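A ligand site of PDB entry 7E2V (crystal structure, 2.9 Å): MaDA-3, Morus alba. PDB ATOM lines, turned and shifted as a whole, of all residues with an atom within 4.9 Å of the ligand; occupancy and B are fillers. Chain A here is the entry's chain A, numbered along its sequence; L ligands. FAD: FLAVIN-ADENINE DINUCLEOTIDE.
An oxygen (O3B) of the ligand sits at hydrogen-bond distance from the guanidinium group (NH2) of Arg 487 (3.3 Å). The backbone NH (N) of Tyr 192 is in hydrogen-bond range of an oxygen (O2) of the ligand, 3.2 Å away. An oxygen (O1P) of the ligand is in hydrogen-bond range of the backbone NH (N) of Gly 185, 3.1 Å away. The side-chain amide nitrogen of Asn 485 is in hydrogen-bond range of an oxygen (O2') of the ligand, at 2.7 Å. The backbone carbonyl oxygen (O) of Gly 185 lies within hydrogen-bond range of an oxygen (O4') of the ligand (3.3 Å). O of His 116 sits at hydrogen-bond distance from O3' of the ligand (3.4 Å). O of Tyr 192 is in hydrogen-bond range of N3 of the ligand (3.0 Å). N of Val 243 sits at hydrogen-bond distance from N1A of the ligand. N of Met 186 lies within hydrogen-bond range of O5' of the ligand, at 3.2 Å. N of Val 177 is in hydrogen-bond range of O4 of the ligand (3.1 Å). N of Gly 238 sits close to N3A of the ligand (3.5 Å). The backbone NH (N) of Ser 113 is in hydrogen-bond range of an oxygen (O2A) of the ligand (2.8 Å). OG of Ser 122 sits at hydrogen-bond distance from O1A of the ligand. N of Gly 115 sits at hydrogen-bond distance from O2A of the ligand (2.9 Å). The backbone carbonyl oxygen (O) of Ile 111 sits at hydrogen-bond distance from an oxygen (O2B) of the ligand, at 3.0 Å. A carbon (C8M) of the ligand is covalently linked to a ring nitrogen (ND1) of His 116 (1.4 Å). An oxygen (O1A) of the ligand sits at hydrogen-bond distance from the backbone NH (N) of Asp 117, at 2.7 Å. N6A of the ligand is in hydrogen-bond range of O of Val 243 (2.8 Å). O1P of the ligand lies close to O of Gly 182, 2.9 Å away. OG of Ser 113 lies within hydrogen-bond range of N7A of the ligand, 2.7 Å away. An oxygen (O1A) of the ligand lies within hydrogen-bond range of the backbone NH (N) of His 116 (2.9 Å). N of Gly 182 sits close to O1P of the ligand, 3.3 Å away. The backbone NH (N) of Gly 114 lies within hydrogen-bond range of an oxygen (O2A) of the ligand, at 3.1 Å.
The backbone NH (N) of Leu 134 sits at hydrogen-bond distance from the backbone carbonyl oxygen (O) of Arg 112, 3.1 Å away. The side-chain hydroxyl (OG) of Ser 113 sits at hydrogen-bond distance from the backbone carbonyl oxygen (O) of Ser 153 (3.2 Å). O of Val 243 sits at hydrogen-bond distance from OG of Ser 153, 3.1 Å away. OH of Tyr 118 is in hydrogen-bond range of NH1 of Arg 443, at 3.0 Å. The backbone NH (N) of Gly 184 lies within hydrogen-bond range of the backbone carbonyl oxygen (O) of Ser 153, at 3.2 Å. The side-chain carboxylate of Asp 117 lies within salt-bridge range of the guanidinium group of Arg 487 (3.1 Å).
The side-chain hydroxyl (OH) of Tyr 118 sits close to a nitrogen (N10) of the ligand (3.4 Å). Merely in contact with the ligand: Arg 112, Leu 134, Ser 153, Val 176, Gly 178, Val 181, Gly 184, Gly 191, Phe 483 and Phe 486. Hydrophobic or aromatic side chains within 4 Å of the ligand: Ile 111, His 116, Tyr 118, Leu 134, Val 176, Val 177, Val 181, Tyr 192, Val 243, Phe 483 and Phe 486. 27 residues have an atom within 4 Å of the ligand: Ile 111, Arg 112, Ser 113, Gly 114, Gly 115, His 116, Asp 117, Tyr 118, Ser 122, Leu 134, Ser 153, Val 176, Val 177, Gly 178, Val 181, Gly 182, Gly 184, Gly 185, Met 186, Gly 191, Tyr 192, Gly 238, Val 243, Phe 483, Asn 485, Phe 486 and Arg 487. Along chain A the residues within 4 Å of the ligand span positions 111 to 487.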
ATOM      1  N   ARG A 110     -16.679  -8.719  10.552  1.00  0.00           N
ATOM      2  CA  ARG A 110     -17.591  -9.694  11.153  1.00  0.00           C
ATOM      3  C   ARG A 110     -17.314 -11.036  10.497  1.00  0.00           C
ATOM      4  O   ARG A 110     -17.715 -11.272   9.347  1.00  0.00           O
ATOM      5  CB  ARG A 110     -19.044  -9.293  10.973  1.00  0.00           C
ATOM      6  CG  ARG A 110     -19.465  -8.168  11.894  1.00  0.00           C
ATOM      7  CD  ARG A 110     -19.101  -8.486  13.329  1.00  0.00           C
ATOM      8  NE  ARG A 110     -19.350  -7.353  14.216  1.00  0.00           N
ATOM      9  CZ  ARG A 110     -20.456  -7.191  14.934  1.00  0.00           C
ATOM     10  NH1 ARG A 110     -21.420  -8.087  14.869  1.00  0.00           N
ATOM     11  NH2 ARG A 110     -20.575  -6.127  15.720  1.00  0.00           N
ATOM     12  N   ILE A 111     -16.648 -11.930  11.217  1.00  0.00           N
ATOM     13  CA  ILE A 111     -16.268 -13.213  10.644  1.00  0.00           C
ATOM     14  C   ILE A 111     -17.525 -14.056  10.499  1.00  0.00           C
ATOM     15  O   ILE A 111     -18.374 -14.080  11.392  1.00  0.00           O
ATOM     16  CB  ILE A 111     -15.262 -13.935  11.540  1.00  0.00           C
ATOM     17  CG1 ILE A 111     -14.047 -13.059  11.809  1.00  0.00           C
ATOM     18  CG2 ILE A 111     -14.775 -15.184  10.830  1.00  0.00           C
ATOM     19  CD1 ILE A 111     -13.228 -13.568  12.973  1.00  0.00           C
ATOM     20  N   ARG A 112     -17.691 -14.701   9.345  1.00  0.00           N
ATOM     21  CA  ARG A 112     -18.851 -15.551   9.148  1.00  0.00           C
ATOM     22  C   ARG A 112     -18.427 -16.841   8.467  1.00  0.00           C
ATOM     23  O   ARG A 112     -17.757 -16.808   7.424  1.00  0.00           O
ATOM     24  CB  ARG A 112     -19.933 -14.831   8.310  1.00  0.00           C
ATOM     25  CG  ARG A 112     -21.251 -15.606   8.243  1.00  0.00           C
ATOM     26  CD  ARG A 112     -22.347 -14.773   7.565  1.00  0.00           C
ATOM     27  NE  ARG A 112     -22.155 -14.730   6.123  1.00  0.00           N
ATOM     28  CZ  ARG A 112     -22.837 -13.944   5.294  1.00  0.00           C
ATOM     29  NH1 ARG A 112     -23.781 -13.130   5.752  1.00  0.00           N
ATOM     30  NH2 ARG A 112     -22.582 -13.977   3.989  1.00  0.00           N
ATOM     31  N   SER A 113     -18.798 -17.970   9.061  1.00  0.00           N
ATOM     32  CA  SER A 113     -18.629 -19.299   8.469  1.00  0.00           C
ATOM     33  C   SER A 113     -19.946 -19.860   7.936  1.00  0.00           C
ATOM     34  O   SER A 113     -20.055 -20.176   6.744  1.00  0.00           O
ATOM     35  CB  SER A 113     -18.025 -20.281   9.484  1.00  0.00           C
ATOM     36  OG  SER A 113     -16.655 -20.037   9.728  1.00  0.00           O
ATOM     37  N   GLY A 114     -20.945 -19.986   8.803  1.00  0.00           N
ATOM     38  CA  GLY A 114     -22.186 -20.615   8.391  1.00  0.00           C
ATOM     39  C   GLY A 114     -23.383 -19.698   8.508  1.00  0.00           C
ATOM     40  O   GLY A 114     -24.428 -19.954   7.918  1.00  0.00           O
ATOM     41  N   GLY A 115     -23.254 -18.624   9.289  1.00  0.00           N
ATOM     42  CA  GLY A 115     -24.328 -17.671   9.445  1.00  0.00           C
ATOM     43  C   GLY A 115     -25.416 -18.062  10.432  1.00  0.00           C
ATOM     44  O   GLY A 115     -26.477 -17.428  10.431  1.00  0.00           O
ATOM     45  N   HIS A 116     -25.197 -19.090  11.246  1.00  0.00           N
ATOM     46  CA  HIS A 116     -26.212 -19.576  12.167  1.00  0.00           C
ATOM     47  C   HIS A 116     -26.282 -18.801  13.473  1.00  0.00           C
ATOM     48  O   HIS A 116     -27.083 -19.179  14.345  1.00  0.00           O
ATOM     49  CB  HIS A 116     -25.999 -21.060  12.474  1.00  0.00           C
ATOM     50  CG  HIS A 116     -26.727 -21.963  11.543  1.00  0.00           C
ATOM     51  ND1 HIS A 116     -28.079 -22.239  11.655  1.00  0.00           N
ATOM     52  CD2 HIS A 116     -26.295 -22.660  10.460  1.00  0.00           C
ATOM     53  CE1 HIS A 116     -28.446 -23.042  10.674  1.00  0.00           C
ATOM     54  NE2 HIS A 116     -27.378 -23.328   9.941  1.00  0.00           N
ATOM     55  N   ASP A 117     -25.425 -17.794  13.665  1.00  0.00           N
ATOM     56  CA  ASP A 117     -25.453 -16.967  14.861  1.00  0.00           C
ATOM     57  C   ASP A 117     -26.881 -16.579  15.244  1.00  0.00           C
ATOM     58  O   ASP A 117     -27.594 -15.947  14.459  1.00  0.00           O
ATOM     59  CB  ASP A 117     -24.606 -15.717  14.659  1.00  0.00           C
ATOM     60  CG  ASP A 117     -24.283 -15.025  15.967  1.00  0.00           C
ATOM     61  OD1 ASP A 117     -25.158 -14.308  16.489  1.00  0.00           O
ATOM     62  OD2 ASP A 117     -23.155 -15.197  16.477  1.00  0.00           O
ATOM     63  N   TYR A 118     -27.279 -16.958  16.451  1.00  0.00           N
ATOM     64  CA  TYR A 118     -28.645 -16.696  16.896  1.00  0.00           C
ATOM     65  C   TYR A 118     -28.960 -15.207  16.877  1.00  0.00           C
ATOM     66  O   TYR A 118     -30.086 -14.814  16.554  1.00  0.00           O
ATOM     67  CB  TYR A 118     -28.858 -17.299  18.288  1.00  0.00           C
ATOM     68  CG  TYR A 118     -29.019 -18.798  18.298  1.00  0.00           C
ATOM     69  CD1 TYR A 118     -29.369 -19.483  17.135  1.00  0.00           C
ATOM     70  CD2 TYR A 118     -28.824 -19.537  19.452  1.00  0.00           C
ATOM     71  CE1 TYR A 118     -29.519 -20.842  17.121  1.00  0.00           C
ATOM     72  CE2 TYR A 118     -28.973 -20.908  19.451  1.00  0.00           C
ATOM     73  CZ  TYR A 118     -29.325 -21.557  18.281  1.00  0.00           C
ATOM     74  OH  TYR A 118     -29.481 -22.920  18.248  1.00  0.00           O
ATOM     75  N   SER A 122     -22.547 -12.317  12.953  1.00  0.00           N
ATOM     76  CA  SER A 122     -21.591 -12.524  11.873  1.00  0.00           C
ATOM     77  C   SER A 122     -21.963 -11.775  10.601  1.00  0.00           C
ATOM     78  O   SER A 122     -21.144 -11.711   9.676  1.00  0.00           O
ATOM     79  CB  SER A 122     -21.449 -14.015  11.572  1.00  0.00           C
ATOM     80  OG  SER A 122     -22.704 -14.604  11.273  1.00  0.00           O
ATOM     81  N   LEU A 134     -16.330 -17.146   4.748  1.00  0.00           N
ATOM     82  CA  LEU A 134     -15.413 -18.254   4.557  1.00  0.00           C
ATOM     83  C   LEU A 134     -16.014 -19.407   3.760  1.00  0.00           C
ATOM     84  O   LEU A 134     -15.439 -20.492   3.757  1.00  0.00           O
ATOM     85  CB  LEU A 134     -14.932 -18.772   5.925  1.00  0.00           C
ATOM     86  CG  LEU A 134     -13.735 -18.050   6.545  1.00  0.00           C
ATOM     87  CD1 LEU A 134     -14.000 -16.560   6.746  1.00  0.00           C
ATOM     88  CD2 LEU A 134     -13.380 -18.678   7.871  1.00  0.00           C
ATOM     89  N   SER A 153     -12.636 -23.709   7.871  1.00  0.00           N
ATOM     90  CA  SER A 153     -13.739 -23.289   8.724  1.00  0.00           C
ATOM     91  C   SER A 153     -15.012 -22.964   7.958  1.00  0.00           C
ATOM     92  O   SER A 153     -16.091 -22.942   8.560  1.00  0.00           O
ATOM     93  CB  SER A 153     -13.315 -22.074   9.563  1.00  0.00           C
ATOM     94  OG  SER A 153     -12.510 -22.471  10.663  1.00  0.00           O
ATOM     95  N   VAL A 176     -23.134 -30.341  16.518  1.00  0.00           N
ATOM     96  CA  VAL A 176     -24.463 -29.814  16.786  1.00  0.00           C
ATOM     97  C   VAL A 176     -25.457 -30.559  15.904  1.00  0.00           C
ATOM     98  O   VAL A 176     -25.071 -31.261  14.964  1.00  0.00           O
ATOM     99  CB  VAL A 176     -24.517 -28.294  16.539  1.00  0.00           C
ATOM    100  CG1 VAL A 176     -23.516 -27.581  17.448  1.00  0.00           C
ATOM    101  CG2 VAL A 176     -24.208 -27.990  15.088  1.00  0.00           C
ATOM    102  N   VAL A 177     -26.754 -30.421  16.205  1.00  0.00           N
ATOM    103  CA  VAL A 177     -27.759 -31.135  15.427  1.00  0.00           C
ATOM    104  C   VAL A 177     -27.861 -30.553  14.021  1.00  0.00           C
ATOM    105  O   VAL A 177     -28.010 -31.293  13.044  1.00  0.00           O
ATOM    106  CB  VAL A 177     -29.119 -31.096  16.145  1.00  0.00           C
ATOM    107  CG1 VAL A 177     -30.121 -31.978  15.435  1.00  0.00           C
ATOM    108  CG2 VAL A 177     -28.955 -31.551  17.589  1.00  0.00           C
ATOM    109  N   GLY A 178     -27.749 -29.234  13.895  1.00  0.00           N
ATOM    110  CA  GLY A 178     -27.865 -28.588  12.609  1.00  0.00           C
ATOM    111  C   GLY A 178     -26.644 -28.807  11.749  1.00  0.00           C
ATOM    112  O   GLY A 178     -25.544 -28.359  12.096  1.00  0.00           O
ATOM    113  N   VAL A 181     -24.557 -25.822  10.169  1.00  0.00           N
ATOM    114  CA  VAL A 181     -23.742 -24.994  11.036  1.00  0.00           C
ATOM    115  C   VAL A 181     -22.303 -25.037  10.540  1.00  0.00           C
ATOM    116  O   VAL A 181     -21.727 -26.111  10.331  1.00  0.00           O
ATOM    117  CB  VAL A 181     -23.837 -25.479  12.492  1.00  0.00           C
ATOM    118  CG1 VAL A 181     -22.810 -24.786  13.344  1.00  0.00           C
ATOM    119  CG2 VAL A 181     -25.211 -25.234  13.062  1.00  0.00           C
ATOM    120  N   GLY A 182     -21.717 -23.855  10.317  1.00  0.00           N
ATOM    121  CA  GLY A 182     -20.322 -23.795   9.929  1.00  0.00           C
ATOM    122  C   GLY A 182     -19.402 -24.259  11.041  1.00  0.00           C
ATOM    123  O   GLY A 182     -19.667 -24.064  12.227  1.00  0.00           O
ATOM    124  N   ILE A 183     -18.286 -24.871  10.634  1.00  0.00           N
ATOM    125  CA  ILE A 183     -17.334 -25.375  11.616  1.00  0.00           C
ATOM    126  C   ILE A 183     -16.697 -24.222  12.380  1.00  0.00           C
ATOM    127  O   ILE A 183     -16.428 -24.329  13.584  1.00  0.00           O
ATOM    128  CB  ILE A 183     -16.285 -26.277  10.952  1.00  0.00           C
ATOM    129  CG1 ILE A 183     -16.946 -27.542  10.392  1.00  0.00           C
ATOM    130  CG2 ILE A 183     -15.160 -26.627  11.920  1.00  0.00           C
ATOM    131  CD1 ILE A 183     -17.989 -28.180  11.312  1.00  0.00           C
ATOM    132  N   GLY A 184     -16.446 -23.103  11.708  1.00  0.00           N
ATOM    133  CA  GLY A 184     -15.783 -21.981  12.343  1.00  0.00           C
ATOM    134  C   GLY A 184     -16.476 -21.461  13.580  1.00  0.00           C
ATOM    135  O   GLY A 184     -15.939 -21.593  14.684  1.00  0.00           O
ATOM    136  N   GLY A 185     -17.664 -20.879  13.427  1.00  0.00           N
ATOM    137  CA  GLY A 185     -18.358 -20.336  14.585  1.00  0.00           C
ATOM    138  C   GLY A 185     -18.788 -21.391  15.577  1.00  0.00           C
ATOM    139  O   GLY A 185     -18.816 -21.144  16.795  1.00  0.00           O
ATOM    140  N   MET A 186     -19.096 -22.596  15.085  1.00  0.00           N
ATOM    141  CA  MET A 186     -19.480 -23.694  15.976  1.00  0.00           C
ATOM    142  C   MET A 186     -18.349 -24.041  16.931  1.00  0.00           C
ATOM    143  O   MET A 186     -18.534 -24.058  18.150  1.00  0.00           O
ATOM    144  CB  MET A 186     -19.867 -24.920  15.171  1.00  0.00           C
ATOM    145  CG  MET A 186     -19.712 -26.197  15.933  1.00  0.00           C
ATOM    146  SD  MET A 186     -19.970 -27.628  14.887  1.00  0.00           S
ATOM    147  CE  MET A 186     -20.397 -28.812  16.143  1.00  0.00           C
ATOM    148  N   ALA A 189     -17.633 -21.293  19.457  1.00  0.00           N
ATOM    149  CA  ALA A 189     -18.392 -21.518  20.668  1.00  0.00           C
ATOM    150  C   ALA A 189     -18.168 -22.983  21.053  1.00  0.00           C
ATOM    151  O   ALA A 189     -17.277 -23.652  20.526  1.00  0.00           O
ATOM    152  CB  ALA A 189     -19.863 -21.166  20.462  1.00  0.00           C
ATOM    153  N   GLY A 191     -20.361 -26.102  21.238  1.00  0.00           N
ATOM    154  CA  GLY A 191     -20.931 -27.162  20.421  1.00  0.00           C
ATOM    155  C   GLY A 191     -21.411 -28.350  21.223  1.00  0.00           C
ATOM    156  O   GLY A 191     -20.615 -29.060  21.850  1.00  0.00           O
ATOM    157  N   TYR A 192     -22.703 -28.624  21.133  1.00  0.00           N
ATOM    158  CA  TYR A 192     -23.358 -29.690  21.877  1.00  0.00           C
ATOM    159  C   TYR A 192     -24.212 -30.509  20.935  1.00  0.00           C
ATOM    160  O   TYR A 192     -24.894 -29.965  20.063  1.00  0.00           O
ATOM    161  CB  TYR A 192     -24.222 -29.117  23.017  1.00  0.00           C
ATOM    162  CG  TYR A 192     -24.912 -30.157  23.863  1.00  0.00           C
ATOM    163  CD1 TYR A 192     -26.157 -30.656  23.519  1.00  0.00           C
ATOM    164  CD2 TYR A 192     -24.316 -30.648  25.017  1.00  0.00           C
ATOM    165  CE1 TYR A 192     -26.794 -31.600  24.283  1.00  0.00           C
ATOM    166  CE2 TYR A 192     -24.935 -31.604  25.801  1.00  0.00           C
ATOM    167  CZ  TYR A 192     -26.177 -32.077  25.418  1.00  0.00           C
ATOM    168  OH  TYR A 192     -26.814 -33.021  26.182  1.00  0.00           O
ATOM    169  N   ALA A 237     -13.954 -16.857  19.819  1.00  0.00           N
ATOM    170  CA  ALA A 237     -12.799 -17.025  18.947  1.00  0.00           C
ATOM    171  C   ALA A 237     -12.707 -15.908  17.929  1.00  0.00           C
ATOM    172  O   ALA A 237     -11.607 -15.528  17.510  1.00  0.00           O
ATOM    173  CB  ALA A 237     -12.860 -18.390  18.253  1.00  0.00           C
ATOM    174  N   GLY A 238     -13.857 -15.376  17.507  1.00  0.00           N
ATOM    175  CA  GLY A 238     -13.881 -14.216  16.634  1.00  0.00           C
ATOM    176  C   GLY A 238     -13.273 -12.976  17.238  1.00  0.00           C
ATOM    177  O   GLY A 238     -12.889 -12.057  16.505  1.00  0.00           O
ATOM    178  N   GLY A 241      -9.036 -13.561  16.691  1.00  0.00           N
ATOM    179  CA  GLY A 241      -8.437 -13.687  15.374  1.00  0.00           C
ATOM    180  C   GLY A 241      -9.435 -14.302  14.421  1.00  0.00           C
ATOM    181  O   GLY A 241     -10.625 -14.418  14.724  1.00  0.00           O
ATOM    182  N   ILE A 242      -8.928 -14.706  13.259  1.00  0.00           N
ATOM    183  CA  ILE A 242      -9.734 -15.349  12.230  1.00  0.00           C
ATOM    184  C   ILE A 242      -9.190 -16.758  12.053  1.00  0.00           C
ATOM    185  O   ILE A 242      -8.069 -16.933  11.568  1.00  0.00           O
ATOM    186  CB  ILE A 242      -9.687 -14.592  10.900  1.00  0.00           C
ATOM    187  CG1 ILE A 242     -10.563 -13.350  10.930  1.00  0.00           C
ATOM    188  CG2 ILE A 242     -10.161 -15.482   9.758  1.00  0.00           C
ATOM    189  CD1 ILE A 242     -10.203 -12.367   9.847  1.00  0.00           C
ATOM    190  N   VAL A 243      -9.983 -17.764  12.419  1.00  0.00           N
ATOM    191  CA  VAL A 243      -9.498 -19.139  12.413  1.00  0.00           C
ATOM    192  C   VAL A 243      -9.843 -19.750  11.061  1.00  0.00           C
ATOM    193  O   VAL A 243     -11.012 -19.786  10.664  1.00  0.00           O
ATOM    194  CB  VAL A 243     -10.079 -19.958  13.561  1.00  0.00           C
ATOM    195  CG1 VAL A 243      -9.291 -21.271  13.714  1.00  0.00           C
ATOM    196  CG2 VAL A 243     -10.058 -19.157  14.854  1.00  0.00           C
ATOM    197  N   ARG A 443     -33.458 -24.805  27.314  1.00  0.00           N
ATOM    198  CA  ARG A 443     -33.497 -23.851  26.223  1.00  0.00           C
ATOM    199  C   ARG A 443     -34.916 -23.354  26.033  1.00  0.00           C
ATOM    200  O   ARG A 443     -35.841 -24.165  25.926  1.00  0.00           O
ATOM    201  CB  ARG A 443     -32.948 -24.495  24.941  1.00  0.00           C
ATOM    202  CG  ARG A 443     -32.756 -23.518  23.794  1.00  0.00           C
ATOM    203  CD  ARG A 443     -31.743 -24.012  22.782  1.00  0.00           C
ATOM    204  NE  ARG A 443     -32.325 -24.972  21.861  1.00  0.00           N
ATOM    205  CZ  ARG A 443     -31.773 -25.322  20.705  1.00  0.00           C
ATOM    206  NH1 ARG A 443     -30.622 -24.787  20.342  1.00  0.00           N
ATOM    207  NH2 ARG A 443     -32.368 -26.206  19.921  1.00  0.00           N
ATOM    208  N   PHE A 483     -25.083 -20.952  27.648  1.00  0.00           N
ATOM    209  CA  PHE A 483     -24.215 -21.653  26.717  1.00  0.00           C
ATOM    210  C   PHE A 483     -23.902 -20.751  25.528  1.00  0.00           C
ATOM    211  O   PHE A 483     -24.808 -20.115  24.974  1.00  0.00           O
ATOM    212  CB  PHE A 483     -24.890 -22.950  26.276  1.00  0.00           C
ATOM    213  CG  PHE A 483     -24.005 -23.892  25.533  1.00  0.00           C
ATOM    214  CD1 PHE A 483     -22.898 -24.451  26.157  1.00  0.00           C
ATOM    215  CD2 PHE A 483     -24.337 -24.323  24.276  1.00  0.00           C
ATOM    216  CE1 PHE A 483     -22.100 -25.367  25.489  1.00  0.00           C
ATOM    217  CE2 PHE A 483     -23.560 -25.240  23.615  1.00  0.00           C
ATOM    218  CZ  PHE A 483     -22.439 -25.754  24.225  1.00  0.00           C
ATOM    219  N   ASN A 485     -22.885 -21.252  22.427  1.00  0.00           N
ATOM    220  CA  ASN A 485     -23.524 -21.566  21.155  1.00  0.00           C
ATOM    221  C   ASN A 485     -24.955 -21.051  21.103  1.00  0.00           C
ATOM    222  O   ASN A 485     -25.477 -20.800  20.011  1.00  0.00           O
ATOM    223  CB  ASN A 485     -23.487 -23.078  20.902  1.00  0.00           C
ATOM    224  CG  ASN A 485     -22.164 -23.552  20.335  1.00  0.00           C
ATOM    225  OD1 ASN A 485     -21.328 -24.089  21.050  1.00  0.00           O
ATOM    226  ND2 ASN A 485     -21.982 -23.381  19.029  1.00  0.00           N
ATOM    227  N   PHE A 486     -25.619 -20.886  22.250  1.00  0.00           N
ATOM    228  CA  PHE A 486     -26.953 -20.281  22.288  1.00  0.00           C
ATOM    229  C   PHE A 486     -26.826 -18.789  22.612  1.00  0.00           C
ATOM    230  O   PHE A 486     -27.153 -18.336  23.706  1.00  0.00           O
ATOM    231  CB  PHE A 486     -27.840 -20.982  23.312  1.00  0.00           C
ATOM    232  CG  PHE A 486     -27.879 -22.484  23.189  1.00  0.00           C
ATOM    233  CD1 PHE A 486     -27.906 -23.265  24.336  1.00  0.00           C
ATOM    234  CD2 PHE A 486     -27.867 -23.105  21.952  1.00  0.00           C
ATOM    235  CE1 PHE A 486     -27.926 -24.633  24.251  1.00  0.00           C
ATOM    236  CE2 PHE A 486     -27.882 -24.482  21.868  1.00  0.00           C
ATOM    237  CZ  PHE A 486     -27.915 -25.254  23.015  1.00  0.00           C
ATOM    238  N   ARG A 487     -26.347 -18.038  21.618  1.00  0.00           N
ATOM    239  CA  ARG A 487     -26.043 -16.633  21.863  1.00  0.00           C
ATOM    240  C   ARG A 487     -27.303 -15.853  22.202  1.00  0.00           C
ATOM    241  O   ARG A 487     -28.378 -16.069  21.634  1.00  0.00           O
ATOM    242  CB  ARG A 487     -25.353 -15.995  20.657  1.00  0.00           C
ATOM    243  CG  ARG A 487     -24.509 -14.789  21.055  1.00  0.00           C
ATOM    244  CD  ARG A 487     -24.134 -13.893  19.879  1.00  0.00           C
ATOM    245  NE  ARG A 487     -22.816 -14.188  19.338  1.00  0.00           N
ATOM    246  CZ  ARG A 487     -21.669 -13.971  19.980  1.00  0.00           C
ATOM    247  NH1 ARG A 487     -21.652 -13.452  21.188  1.00  0.00           N
ATOM    248  NH2 ARG A 487     -20.510 -14.279  19.385  1.00  0.00           N
ATOM    249  N   TYR A 540     -16.877  -7.029  18.950  1.00  0.00           N
ATOM    250  CA  TYR A 540     -18.293  -7.136  18.583  1.00  0.00           C
ATOM    251  C   TYR A 540     -19.150  -7.077  19.857  1.00  0.00           C
ATOM    252  O   TYR A 540     -18.670  -6.704  20.930  1.00  0.00           O
ATOM    253  CB  TYR A 540     -18.562  -8.414  17.763  1.00  0.00           C
ATOM    254  CG  TYR A 540     -18.022  -9.698  18.341  1.00  0.00           C
ATOM    255  CD1 TYR A 540     -16.712 -10.117  18.077  1.00  0.00           C
ATOM    256  CD2 TYR A 540     -18.846 -10.516  19.136  1.00  0.00           C
ATOM    257  CE1 TYR A 540     -16.218 -11.299  18.593  1.00  0.00           C
ATOM    258  CE2 TYR A 540     -18.367 -11.708  19.659  1.00  0.00           C
ATOM    259  CZ  TYR A 540     -17.051 -12.087  19.384  1.00  0.00           C
ATOM    260  OH  TYR A 540     -16.570 -13.266  19.903  1.00  0.00           O
HETATM  261  PA  FAD L   1     -21.507 -17.819  12.268  1.00  0.00           P
HETATM  262  O1A FAD L   1     -22.974 -17.702  12.424  1.00  0.00           O
HETATM  263  O2A FAD L   1     -20.991 -17.700  10.826  1.00  0.00           O
HETATM  264  O5B FAD L   1     -20.803 -16.811  13.215  1.00  0.00           O
HETATM  265  C5B FAD L   1     -21.187 -16.708  14.599  1.00  0.00           C
HETATM  266  C4B FAD L   1     -20.001 -16.353  15.466  1.00  0.00           C
HETATM  267  O4B FAD L   1     -18.872 -17.186  15.104  1.00  0.00           O
HETATM  268  C3B FAD L   1     -19.498 -14.913  15.329  1.00  0.00           C
HETATM  269  O3B FAD L   1     -18.925 -14.463  16.549  1.00  0.00           O
HETATM  270  C2B FAD L   1     -18.415 -15.059  14.249  1.00  0.00           C
HETATM  271  O2B FAD L   1     -17.492 -13.972  14.253  1.00  0.00           O
HETATM  272  C1B FAD L   1     -17.791 -16.371  14.689  1.00  0.00           C
HETATM  273  N9A FAD L   1     -17.041 -17.081  13.659  1.00  0.00           N
HETATM  274  C8A FAD L   1     -17.524 -17.734  12.563  1.00  0.00           C
HETATM  275  N7A FAD L   1     -16.606 -18.291  11.810  1.00  0.00           N
HETATM  276  C5A FAD L   1     -15.411 -17.980  12.468  1.00  0.00           C
HETATM  277  C6A FAD L   1     -14.077 -18.262  12.177  1.00  0.00           C
HETATM  278  N6A FAD L   1     -13.663 -18.970  11.122  1.00  0.00           N
HETATM  279  N1A FAD L   1     -13.131 -17.804  13.042  1.00  0.00           N
HETATM  280  C2A FAD L   1     -13.536 -17.102  14.105  1.00  0.00           C
HETATM  281  N3A FAD L   1     -14.771 -16.764  14.471  1.00  0.00           N
HETATM  282  C4A FAD L   1     -15.682 -17.234  13.609  1.00  0.00           C
HETATM  283  N1  FAD L   1     -25.522 -25.048  18.948  1.00  0.00           N
HETATM  284  C2  FAD L   1     -25.384 -26.094  19.814  1.00  0.00           C
HETATM  285  O2  FAD L   1     -24.622 -26.038  20.784  1.00  0.00           O
HETATM  286  N3  FAD L   1     -26.106 -27.251  19.613  1.00  0.00           N
HETATM  287  C4  FAD L   1     -27.006 -27.486  18.587  1.00  0.00           C
HETATM  288  O4  FAD L   1     -27.585 -28.556  18.515  1.00  0.00           O
HETATM  289  C4X FAD L   1     -27.143 -26.379  17.675  1.00  0.00           C
HETATM  290  N5  FAD L   1     -27.960 -26.508  16.675  1.00  0.00           N
HETATM  291  C5X FAD L   1     -28.106 -25.456  15.800  1.00  0.00           C
HETATM  292  C6  FAD L   1     -28.982 -25.590  14.723  1.00  0.00           C
HETATM  293  C7  FAD L   1     -29.167 -24.564  13.812  1.00  0.00           C
HETATM  294  C7M FAD L   1     -30.131 -24.759  12.679  1.00  0.00           C
HETATM  295  C8  FAD L   1     -28.461 -23.358  13.964  1.00  0.00           C
HETATM  296  C8M FAD L   1     -28.619 -22.231  12.980  1.00  0.00           C
HETATM  297  C9  FAD L   1     -27.578 -23.219  15.038  1.00  0.00           C
HETATM  298  C9A FAD L   1     -27.395 -24.259  15.953  1.00  0.00           C
HETATM  299  N10 FAD L   1     -26.500 -24.148  17.040  1.00  0.00           N
HETATM  300  C10 FAD L   1     -26.364 -25.195  17.927  1.00  0.00           C
HETATM  301  C1' FAD L   1     -25.741 -22.917  17.287  1.00  0.00           C
HETATM  302  C2' FAD L   1     -24.444 -22.829  16.507  1.00  0.00           C
HETATM  303  O2' FAD L   1     -23.531 -23.849  16.908  1.00  0.00           O
HETATM  304  C3' FAD L   1     -23.810 -21.465  16.764  1.00  0.00           C
HETATM  305  O3' FAD L   1     -24.779 -20.458  16.500  1.00  0.00           O
HETATM  306  C4' FAD L   1     -22.568 -21.211  15.910  1.00  0.00           C
HETATM  307  O4' FAD L   1     -21.907 -20.009  16.323  1.00  0.00           O
HETATM  308  C5' FAD L   1     -22.899 -21.160  14.438  1.00  0.00           C
HETATM  309  O5' FAD L   1     -21.706 -21.409  13.668  1.00  0.00           O
HETATM  310  P   FAD L   1     -21.429 -20.630  12.335  1.00  0.00           P
HETATM  311  O1P FAD L   1     -20.221 -21.255  11.635  1.00  0.00           O
HETATM  312  O2P FAD L   1     -22.671 -20.538  11.548  1.00  0.00           O
HETATM  313  O3P FAD L   1     -21.001 -19.198  12.857  1.00  0.00           O
